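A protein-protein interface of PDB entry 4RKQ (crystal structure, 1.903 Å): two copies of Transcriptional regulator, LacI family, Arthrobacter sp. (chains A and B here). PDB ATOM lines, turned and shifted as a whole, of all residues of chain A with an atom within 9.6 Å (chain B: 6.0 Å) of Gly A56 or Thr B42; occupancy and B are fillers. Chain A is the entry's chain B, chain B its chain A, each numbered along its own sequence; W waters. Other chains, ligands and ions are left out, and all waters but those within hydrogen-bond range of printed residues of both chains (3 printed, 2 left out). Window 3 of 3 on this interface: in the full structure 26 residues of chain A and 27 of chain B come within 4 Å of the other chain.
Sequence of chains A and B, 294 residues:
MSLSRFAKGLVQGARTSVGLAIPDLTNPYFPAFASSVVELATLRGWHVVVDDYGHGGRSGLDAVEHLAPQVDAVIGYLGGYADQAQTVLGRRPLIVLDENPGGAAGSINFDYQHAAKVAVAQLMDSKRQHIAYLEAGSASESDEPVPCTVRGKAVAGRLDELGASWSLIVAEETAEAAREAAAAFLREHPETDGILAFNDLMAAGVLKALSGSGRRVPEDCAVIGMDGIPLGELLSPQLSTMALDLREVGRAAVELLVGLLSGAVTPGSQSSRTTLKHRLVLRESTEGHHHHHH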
ATOM      1  N   PRO A  23       3.394 -24.764  -9.915  1.00  0.00           N
ATOM      2  CA  PRO A  23       2.715 -23.478  -9.663  1.00  0.00           C
ATOM      3  C   PRO A  23       2.247 -23.286  -8.246  1.00  0.00           C
ATOM      4  O   PRO A  23       1.947 -22.170  -7.850  1.00  0.00           O
ATOM      5  CB  PRO A  23       1.529 -23.512 -10.633  1.00  0.00           C
ATOM      6  CG  PRO A  23       1.279 -24.934 -10.817  1.00  0.00           C
ATOM      7  CD  PRO A  23       2.618 -25.586 -10.847  1.00  0.00           C
ATOM      8  N   ASP A  51      11.102 -25.242  -7.322  1.00  0.00           N
ATOM      9  CA  ASP A  51      10.661 -23.834  -7.230  1.00  0.00           C
ATOM     10  C   ASP A  51       9.153 -23.837  -7.297  1.00  0.00           C
ATOM     11  O   ASP A  51       8.583 -24.127  -8.338  1.00  0.00           O
ATOM     12  CB  ASP A  51      11.265 -23.013  -8.379  1.00  0.00           C
ATOM     13  CG  ASP A  51      10.919 -21.534  -8.304  1.00  0.00           C
ATOM     14  OD1 ASP A  51      10.017 -21.171  -7.568  1.00  0.00           O
ATOM     15  OD2 ASP A  51      11.574 -20.702  -8.956  1.00  0.00           O
ATOM     16  N   ASP A  52       8.531 -23.541  -6.172  1.00  0.00           N
ATOM     17  CA  ASP A  52       7.107 -23.340  -6.080  1.00  0.00           C
ATOM     18  C   ASP A  52       6.902 -21.852  -6.406  1.00  0.00           C
ATOM     19  O   ASP A  52       7.262 -20.972  -5.629  1.00  0.00           O
ATOM     20  CB  ASP A  52       6.613 -23.658  -4.690  1.00  0.00           C
ATOM     21  CG  ASP A  52       5.245 -23.031  -4.360  1.00  0.00           C
ATOM     22  OD1 ASP A  52       4.537 -22.541  -5.258  1.00  0.00           O
ATOM     23  OD2 ASP A  52       4.896 -22.999  -3.165  1.00  0.00           O
ATOM     24  N   TYR A  53       6.378 -21.588  -7.589  1.00  0.00           N
ATOM     25  CA  TYR A  53       6.248 -20.209  -8.035  1.00  0.00           C
ATOM     26  C   TYR A  53       4.883 -19.555  -7.827  1.00  0.00           C
ATOM     27  O   TYR A  53       4.635 -18.465  -8.375  1.00  0.00           O
ATOM     28  CB  TYR A  53       6.667 -20.095  -9.508  1.00  0.00           C
ATOM     29  CG  TYR A  53       5.827 -20.802 -10.546  1.00  0.00           C
ATOM     30  CD1 TYR A  53       4.685 -20.189 -11.103  1.00  0.00           C
ATOM     31  CD2 TYR A  53       6.214 -22.037 -11.054  1.00  0.00           C
ATOM     32  CE1 TYR A  53       3.935 -20.803 -12.074  1.00  0.00           C
ATOM     33  CE2 TYR A  53       5.464 -22.689 -12.049  1.00  0.00           C
ATOM     34  CZ  TYR A  53       4.330 -22.069 -12.566  1.00  0.00           C
ATOM     35  OH  TYR A  53       3.607 -22.724 -13.540  1.00  0.00           O
ATOM     36  N   GLY A  54       4.023 -20.150  -7.022  1.00  0.00           N
ATOM     37  CA  GLY A  54       2.684 -19.648  -6.829  1.00  0.00           C
ATOM     38  C   GLY A  54       2.640 -18.498  -5.818  1.00  0.00           C
ATOM     39  O   GLY A  54       1.786 -18.480  -4.954  1.00  0.00           O
ATOM     40  N   HIS A  55       3.572 -17.564  -5.893  1.00  0.00           N
ATOM     41  CA  HIS A  55       3.629 -16.512  -4.904  1.00  0.00           C
ATOM     42  C   HIS A  55       4.134 -15.232  -5.553  1.00  0.00           C
ATOM     43  O   HIS A  55       4.864 -15.282  -6.526  1.00  0.00           O
ATOM     44  CB  HIS A  55       4.606 -16.914  -3.812  1.00  0.00           C
ATOM     45  CG  HIS A  55       4.330 -18.254  -3.208  1.00  0.00           C
ATOM     46  ND1 HIS A  55       3.435 -18.424  -2.186  1.00  0.00           N
ATOM     47  CD2 HIS A  55       4.789 -19.494  -3.515  1.00  0.00           C
ATOM     48  CE1 HIS A  55       3.386 -19.694  -1.842  1.00  0.00           C
ATOM     49  NE2 HIS A  55       4.174 -20.369  -2.656  1.00  0.00           N
ATOM     50  N   GLY A  56       3.772 -14.068  -5.008  1.00  0.00           N
ATOM     51  CA  GLY A  56       4.383 -12.791  -5.457  1.00  0.00           C
ATOM     52  C   GLY A  56       4.210 -12.427  -6.929  1.00  0.00           C
ATOM     53  O   GLY A  56       5.072 -11.772  -7.543  1.00  0.00           O
ATOM     54  N   GLY A  57       3.127 -12.906  -7.512  1.00  0.00           N
ATOM     55  CA  GLY A  57       2.892 -12.708  -8.938  1.00  0.00           C
ATOM     56  C   GLY A  57       3.813 -13.421  -9.898  1.00  0.00           C
ATOM     57  O   GLY A  57       3.817 -13.083 -11.072  1.00  0.00           O
ATOM     58  N   ARG A  58       4.587 -14.414  -9.446  1.00  0.00           N
ATOM     59  CA  ARG A  58       5.602 -15.014 -10.336  1.00  0.00           C
ATOM     60  C   ARG A  58       4.930 -15.951 -11.331  1.00  0.00           C
ATOM     61  O   ARG A  58       3.839 -16.466 -11.074  1.00  0.00           O
ATOM     62  CB  ARG A  58       6.652 -15.772  -9.523  1.00  0.00           C
ATOM     63  CG  ARG A  58       7.563 -14.882  -8.714  1.00  0.00           C
ATOM     64  CD  ARG A  58       8.518 -15.639  -7.784  1.00  0.00           C
ATOM     65  NE  ARG A  58       9.574 -16.293  -8.540  1.00  0.00           N
ATOM     66  CZ  ARG A  58       9.896 -17.582  -8.489  1.00  0.00           C
ATOM     67  NH1 ARG A  58       9.295 -18.424  -7.661  1.00  0.00           N
ATOM     68  NH2 ARG A  58      10.840 -18.033  -9.286  1.00  0.00           N
ATOM     69  N   SER A  59       5.616 -16.231 -12.438  1.00  0.00           N
ATOM     70  CA  SER A  59       5.078 -17.103 -13.472  1.00  0.00           C
ATOM     71  C   SER A  59       6.021 -18.295 -13.677  1.00  0.00           C
ATOM     72  O   SER A  59       7.102 -18.347 -13.105  1.00  0.00           O
ATOM     73  CB  SER A  59       4.986 -16.316 -14.784  1.00  0.00           C
ATOM     74  OG  SER A  59       6.299 -16.067 -15.251  1.00  0.00           O
ATOM     75  N   ASP A  62       9.413 -17.083 -14.812  1.00  0.00           N
ATOM     76  CA  ASP A  62      10.240 -16.614 -13.688  1.00  0.00           C
ATOM     77  C   ASP A  62      10.865 -17.807 -13.001  1.00  0.00           C
ATOM     78  O   ASP A  62      12.004 -17.749 -12.588  1.00  0.00           O
ATOM     79  CB  ASP A  62       9.398 -15.863 -12.664  1.00  0.00           C
ATOM     80  CG  ASP A  62       8.858 -14.537 -13.193  1.00  0.00           C
ATOM     81  OD1 ASP A  62       9.551 -13.858 -13.965  1.00  0.00           O
ATOM     82  OD2 ASP A  62       7.735 -14.167 -12.833  1.00  0.00           O
ATOM     83  N   HIS A  66      14.927 -18.423 -12.712  1.00  0.00           N
ATOM     84  CA  HIS A  66      15.556 -18.552 -11.395  1.00  0.00           C
ATOM     85  C   HIS A  66      16.428 -19.829 -11.350  1.00  0.00           C
ATOM     86  O   HIS A  66      17.564 -19.802 -10.894  1.00  0.00           O
ATOM     87  CB  HIS A  66      14.462 -18.570 -10.341  1.00  0.00           C
ATOM     88  CG  HIS A  66      14.882 -19.098  -9.013  1.00  0.00           C
ATOM     89  ND1 HIS A  66      14.085 -19.952  -8.276  1.00  0.00           N
ATOM     90  CD2 HIS A  66      16.017 -18.923  -8.293  1.00  0.00           C
ATOM     91  CE1 HIS A  66      14.699 -20.246  -7.146  1.00  0.00           C
ATOM     92  NE2 HIS A  66      15.864 -19.630  -7.131  1.00  0.00           N
ATOM     93  N   VAL B  37       6.480 -20.591   3.956  1.00  0.00           N
ATOM     94  CA  VAL B  37       7.821 -20.009   3.920  1.00  0.00           C
ATOM     95  C   VAL B  37       8.143 -19.420   2.545  1.00  0.00           C
ATOM     96  O   VAL B  37       8.692 -18.301   2.457  1.00  0.00           O
ATOM     97  CB  VAL B  37       8.948 -21.004   4.338  1.00  0.00           C
ATOM     98  CG1 VAL B  37      10.310 -20.354   4.178  1.00  0.00           C
ATOM     99  CG2 VAL B  37       8.761 -21.457   5.781  1.00  0.00           C
ATOM    100  N   VAL B  38       7.784 -20.123   1.478  1.00  0.00           N
ATOM    101  CA  VAL B  38       8.042 -19.594   0.142  1.00  0.00           C
ATOM    102  C   VAL B  38       7.260 -18.282  -0.099  1.00  0.00           C
ATOM    103  O   VAL B  38       7.816 -17.386  -0.696  1.00  0.00           O
ATOM    104  CB  VAL B  38       7.745 -20.587  -0.958  1.00  0.00           C
ATOM    105  CG1 VAL B  38       7.949 -19.961  -2.300  1.00  0.00           C
ATOM    106  CG2 VAL B  38       8.709 -21.760  -0.846  1.00  0.00           C
ATOM    107  N   GLU B  39       6.012 -18.229   0.352  1.00  0.00           N
ATOM    108  CA  GLU B  39       5.203 -16.996   0.328  1.00  0.00           C
ATOM    109  C   GLU B  39       5.921 -15.800   0.975  1.00  0.00           C
ATOM    110  O   GLU B  39       6.112 -14.761   0.339  1.00  0.00           O
ATOM    111  CB  GLU B  39       3.861 -17.196   1.000  1.00  0.00           C
ATOM    112  CG  GLU B  39       2.979 -15.928   1.120  1.00  0.00           C
ATOM    113  CD  GLU B  39       2.286 -15.491  -0.159  1.00  0.00           C
ATOM    114  OE1 GLU B  39       2.518 -16.090  -1.237  1.00  0.00           O
ATOM    115  OE2 GLU B  39       1.487 -14.521  -0.088  1.00  0.00           O
ATOM    116  N   LEU B  40       6.364 -15.961   2.213  1.00  0.00           N
ATOM    117  CA  LEU B  40       6.951 -14.835   2.953  1.00  0.00           C
ATOM    118  C   LEU B  40       8.277 -14.435   2.374  1.00  0.00           C
ATOM    119  O   LEU B  40       8.553 -13.262   2.257  1.00  0.00           O
ATOM    120  CB  LEU B  40       7.050 -15.147   4.441  1.00  0.00           C
ATOM    121  CG  LEU B  40       5.701 -15.400   5.064  1.00  0.00           C
ATOM    122  CD1 LEU B  40       5.893 -16.121   6.383  1.00  0.00           C
ATOM    123  CD2 LEU B  40       4.936 -14.104   5.229  1.00  0.00           C
ATOM    124  N   ALA B  41       9.088 -15.397   1.927  1.00  0.00           N
ATOM    125  CA  ALA B  41      10.369 -15.101   1.377  1.00  0.00           C
ATOM    126  C   ALA B  41      10.212 -14.414   0.042  1.00  0.00           C
ATOM    127  O   ALA B  41      10.968 -13.475  -0.301  1.00  0.00           O
ATOM    128  CB  ALA B  41      11.217 -16.376   1.222  1.00  0.00           C
ATOM    129  N   THR B  42       9.263 -14.897  -0.744  1.00  0.00           N
ATOM    130  CA  THR B  42       9.061 -14.389  -2.070  1.00  0.00           C
ATOM    131  C   THR B  42       8.620 -12.902  -1.967  1.00  0.00           C
ATOM    132  O   THR B  42       9.030 -12.056  -2.740  1.00  0.00           O
ATOM    133  CB  THR B  42       8.030 -15.234  -2.845  1.00  0.00           C
ATOM    134  OG1 THR B  42       8.592 -16.550  -3.113  1.00  0.00           O
ATOM    135  CG2 THR B  42       7.680 -14.557  -4.139  1.00  0.00           C
ATOM    136  N   LEU B  43       7.813 -12.626  -0.974  1.00  0.00           N
ATOM    137  CA  LEU B  43       7.322 -11.266  -0.763  1.00  0.00           C
ATOM    138  C   LEU B  43       8.394 -10.298  -0.246  1.00  0.00           C
ATOM    139  O   LEU B  43       8.189  -9.071  -0.306  1.00  0.00           O
ATOM    140  CB  LEU B  43       6.157 -11.313   0.149  1.00  0.00           C
ATOM    141  CG  LEU B  43       4.879 -11.932  -0.377  1.00  0.00           C
ATOM    142  CD1 LEU B  43       3.832 -11.978   0.747  1.00  0.00           C
ATOM    143  CD2 LEU B  43       4.375 -11.177  -1.579  1.00  0.00           C
ATOM    144  N   ARG B  44       9.533 -10.832   0.225  1.00  0.00           N
ATOM    145  CA  ARG B  44      10.711 -10.027   0.523  1.00  0.00           C
ATOM    146  C   ARG B  44      11.643  -9.922  -0.662  1.00  0.00           C
ATOM    147  O   ARG B  44      12.757  -9.328  -0.541  1.00  0.00           O
ATOM    148  CB  ARG B  44      11.478 -10.593   1.725  1.00  0.00           C
ATOM    149  CG  ARG B  44      10.700 -10.698   3.022  1.00  0.00           C
ATOM    150  CD  ARG B  44      11.643 -11.004   4.161  1.00  0.00           C
ATOM    151  NE  ARG B  44      12.497  -9.860   4.450  1.00  0.00           N
ATOM    152  CZ  ARG B  44      12.173  -8.909   5.332  1.00  0.00           C
ATOM    153  NH1 ARG B  44      11.032  -8.995   6.019  1.00  0.00           N
ATOM    154  NH2 ARG B  44      13.000  -7.894   5.523  1.00  0.00           N
ATOM    155  N   GLY B  45      11.260 -10.452  -1.810  1.00  0.00           N
ATOM    156  CA  GLY B  45      12.110 -10.430  -3.006  1.00  0.00           C
ATOM    157  C   GLY B  45      13.202 -11.481  -3.028  1.00  0.00           C
ATOM    158  O   GLY B  45      14.148 -11.389  -3.800  1.00  0.00           O
ATOM    159  N   TRP B  46      13.104 -12.428  -2.119  1.00  0.00           N
ATOM    160  CA  TRP B  46      14.093 -13.511  -2.008  1.00  0.00           C
ATOM    161  C   TRP B  46      13.806 -14.657  -3.023  1.00  0.00           C
ATOM    162  O   TRP B  46      12.670 -14.869  -3.424  1.00  0.00           O
ATOM    163  CB  TRP B  46      14.036 -14.060  -0.600  1.00  0.00           C
ATOM    164  CG  TRP B  46      14.487 -13.168   0.448  1.00  0.00           C
ATOM    165  CD1 TRP B  46      15.008 -11.897   0.314  1.00  0.00           C
ATOM    166  CD2 TRP B  46      14.557 -13.492   1.841  1.00  0.00           C
ATOM    167  NE1 TRP B  46      15.364 -11.420   1.562  1.00  0.00           N
ATOM    168  CE2 TRP B  46      15.060 -12.360   2.510  1.00  0.00           C
ATOM    169  CE3 TRP B  46      14.188 -14.624   2.596  1.00  0.00           C
ATOM    170  CZ2 TRP B  46      15.262 -12.338   3.881  1.00  0.00           C
ATOM    171  CZ3 TRP B  46      14.342 -14.580   3.963  1.00  0.00           C
ATOM    172  CH2 TRP B  46      14.907 -13.448   4.588  1.00  0.00           C
ATOM    173  N   VAL B  48      13.875 -18.787  -3.411  1.00  0.00           N
ATOM    174  CA  VAL B  48      13.793 -19.952  -2.530  1.00  0.00           C
ATOM    175  C   VAL B  48      13.868 -21.225  -3.389  1.00  0.00           C
ATOM    176  O   VAL B  48      13.245 -21.325  -4.460  1.00  0.00           O
ATOM    177  CB  VAL B  48      12.474 -20.019  -1.728  1.00  0.00           C
ATOM    178  CG1 VAL B  48      12.455 -21.214  -0.776  1.00  0.00           C
ATOM    179  CG2 VAL B  48      12.230 -18.750  -0.931  1.00  0.00           C
HETATM  180  O   HOH W   1      12.177 -18.481  -5.791  1.00  0.00           O
HETATM  181  O   HOH W   2       1.797 -13.950  -2.932  1.00  0.00           O
HETATM  182  O   HOH W   3       7.564 -18.127  -5.426  1.00  0.00           O
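A ring nitrogen (ND1) of His A55 sits at hydrogen-bond distance from the side-chain carboxylate (OE1) of Glu B39 (2.7 Å).
The guanidinium group (NH2) of Arg A58 lies within salt-bridge range of the side-chain carboxylate (OD2) of Asp A51 (2.8 Å). OD1 of Asp A52 sits at hydrogen-bond distance from N of Gly A54 (3.0 Å). The backbone carbonyl oxygen (O) of Val B38 sits at hydrogen-bond distance from the side-chain hydroxyl (OG1) of Thr B42. NE2 of His A55 lies within hydrogen-bond range of OD2 of Asp A52, 2.8 Å away. A ring nitrogen (ND1) of His A66 lies within hydrogen-bond range of the side-chain carboxylate (OD2) of Asp A51, at 2.7 Å.
Among the printed residues, merely in contact across the chains: Asp A52 with Val B38 (3.5 Å), His A55 with Val B38 (3.4 Å), His A55 with Thr B42 (3.8 Å), Gly A56 with Thr B42 (3.97 Å), Arg A58 with Thr B42 (3.9 Å) and His A66 with Val B48 (3.2 Å).
Gly A54 touches none of the printed residues of chain B. Printed residues of chain B within 4 Å of His A55: Val B38, Glu B39 and Thr B42. Of chain B, only Thr B42 (3.97 Å) comes within 4 Å of Gly A56. Ser A59 touches none of the printed residues of chain B. Of the printed residues of chain A, Glu B39 touches His A55 (2.7 Å). Thr B42 touches just these residues of chain A: His A55, Gly A56 and Arg A58. No residue of chain A comes within 4 Å of Gly B45. Printed residues of chain A within 4 Å of Val B48: His A66 (3.2 Å). The nearest residue of chain A that does not touch Thr B42 is Asp A52 (5.3 Å). The nearest printed residue of chain A that does not touch Val B48 is Asp A51 (4.5 Å).
Printed residues of chain A that touch a printed residue of chain B: Asp A52, His A55, Gly A56, Arg A58 and His A66. Hydrophobic or aromatic side chains of chain A within 4 Å of the printed part of chain B: His A55 and His A66. Of the 11 printed residues of chain B, 4 touch a printed residue of chain A. Among the printed residues, 7 pairs touch across the chains. Among the printed residues, no Asp or Glu carboxylate lies within 4 Å of a Lys or Arg side-chain nitrogen of the other chain.
No position is printed for both chains. Of the 7 pairs that touch across the chains among the printed residues, none has its exchanged pair printed and touching as well.
Water W2 lies within hydrogen-bond range of the side-chain carboxylate of Glu B39 (2.8 Å) and the backbone NH of Gly A56 (2.9 Å). Water W3 lies within hydrogen-bond range of the guanidinium group (NH1) of Arg A58 (2.8 Å), the backbone carbonyl oxygen (O) of Asp A52 (2.9 Å) and the side-chain hydroxyl (OG1) of Thr B42 (3.0 Å). Water W1 lies within hydrogen-bond range of the backbone NH of Val B48, the guanidinium group of Arg A58 and a ring nitrogen (ND1) of His A66.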
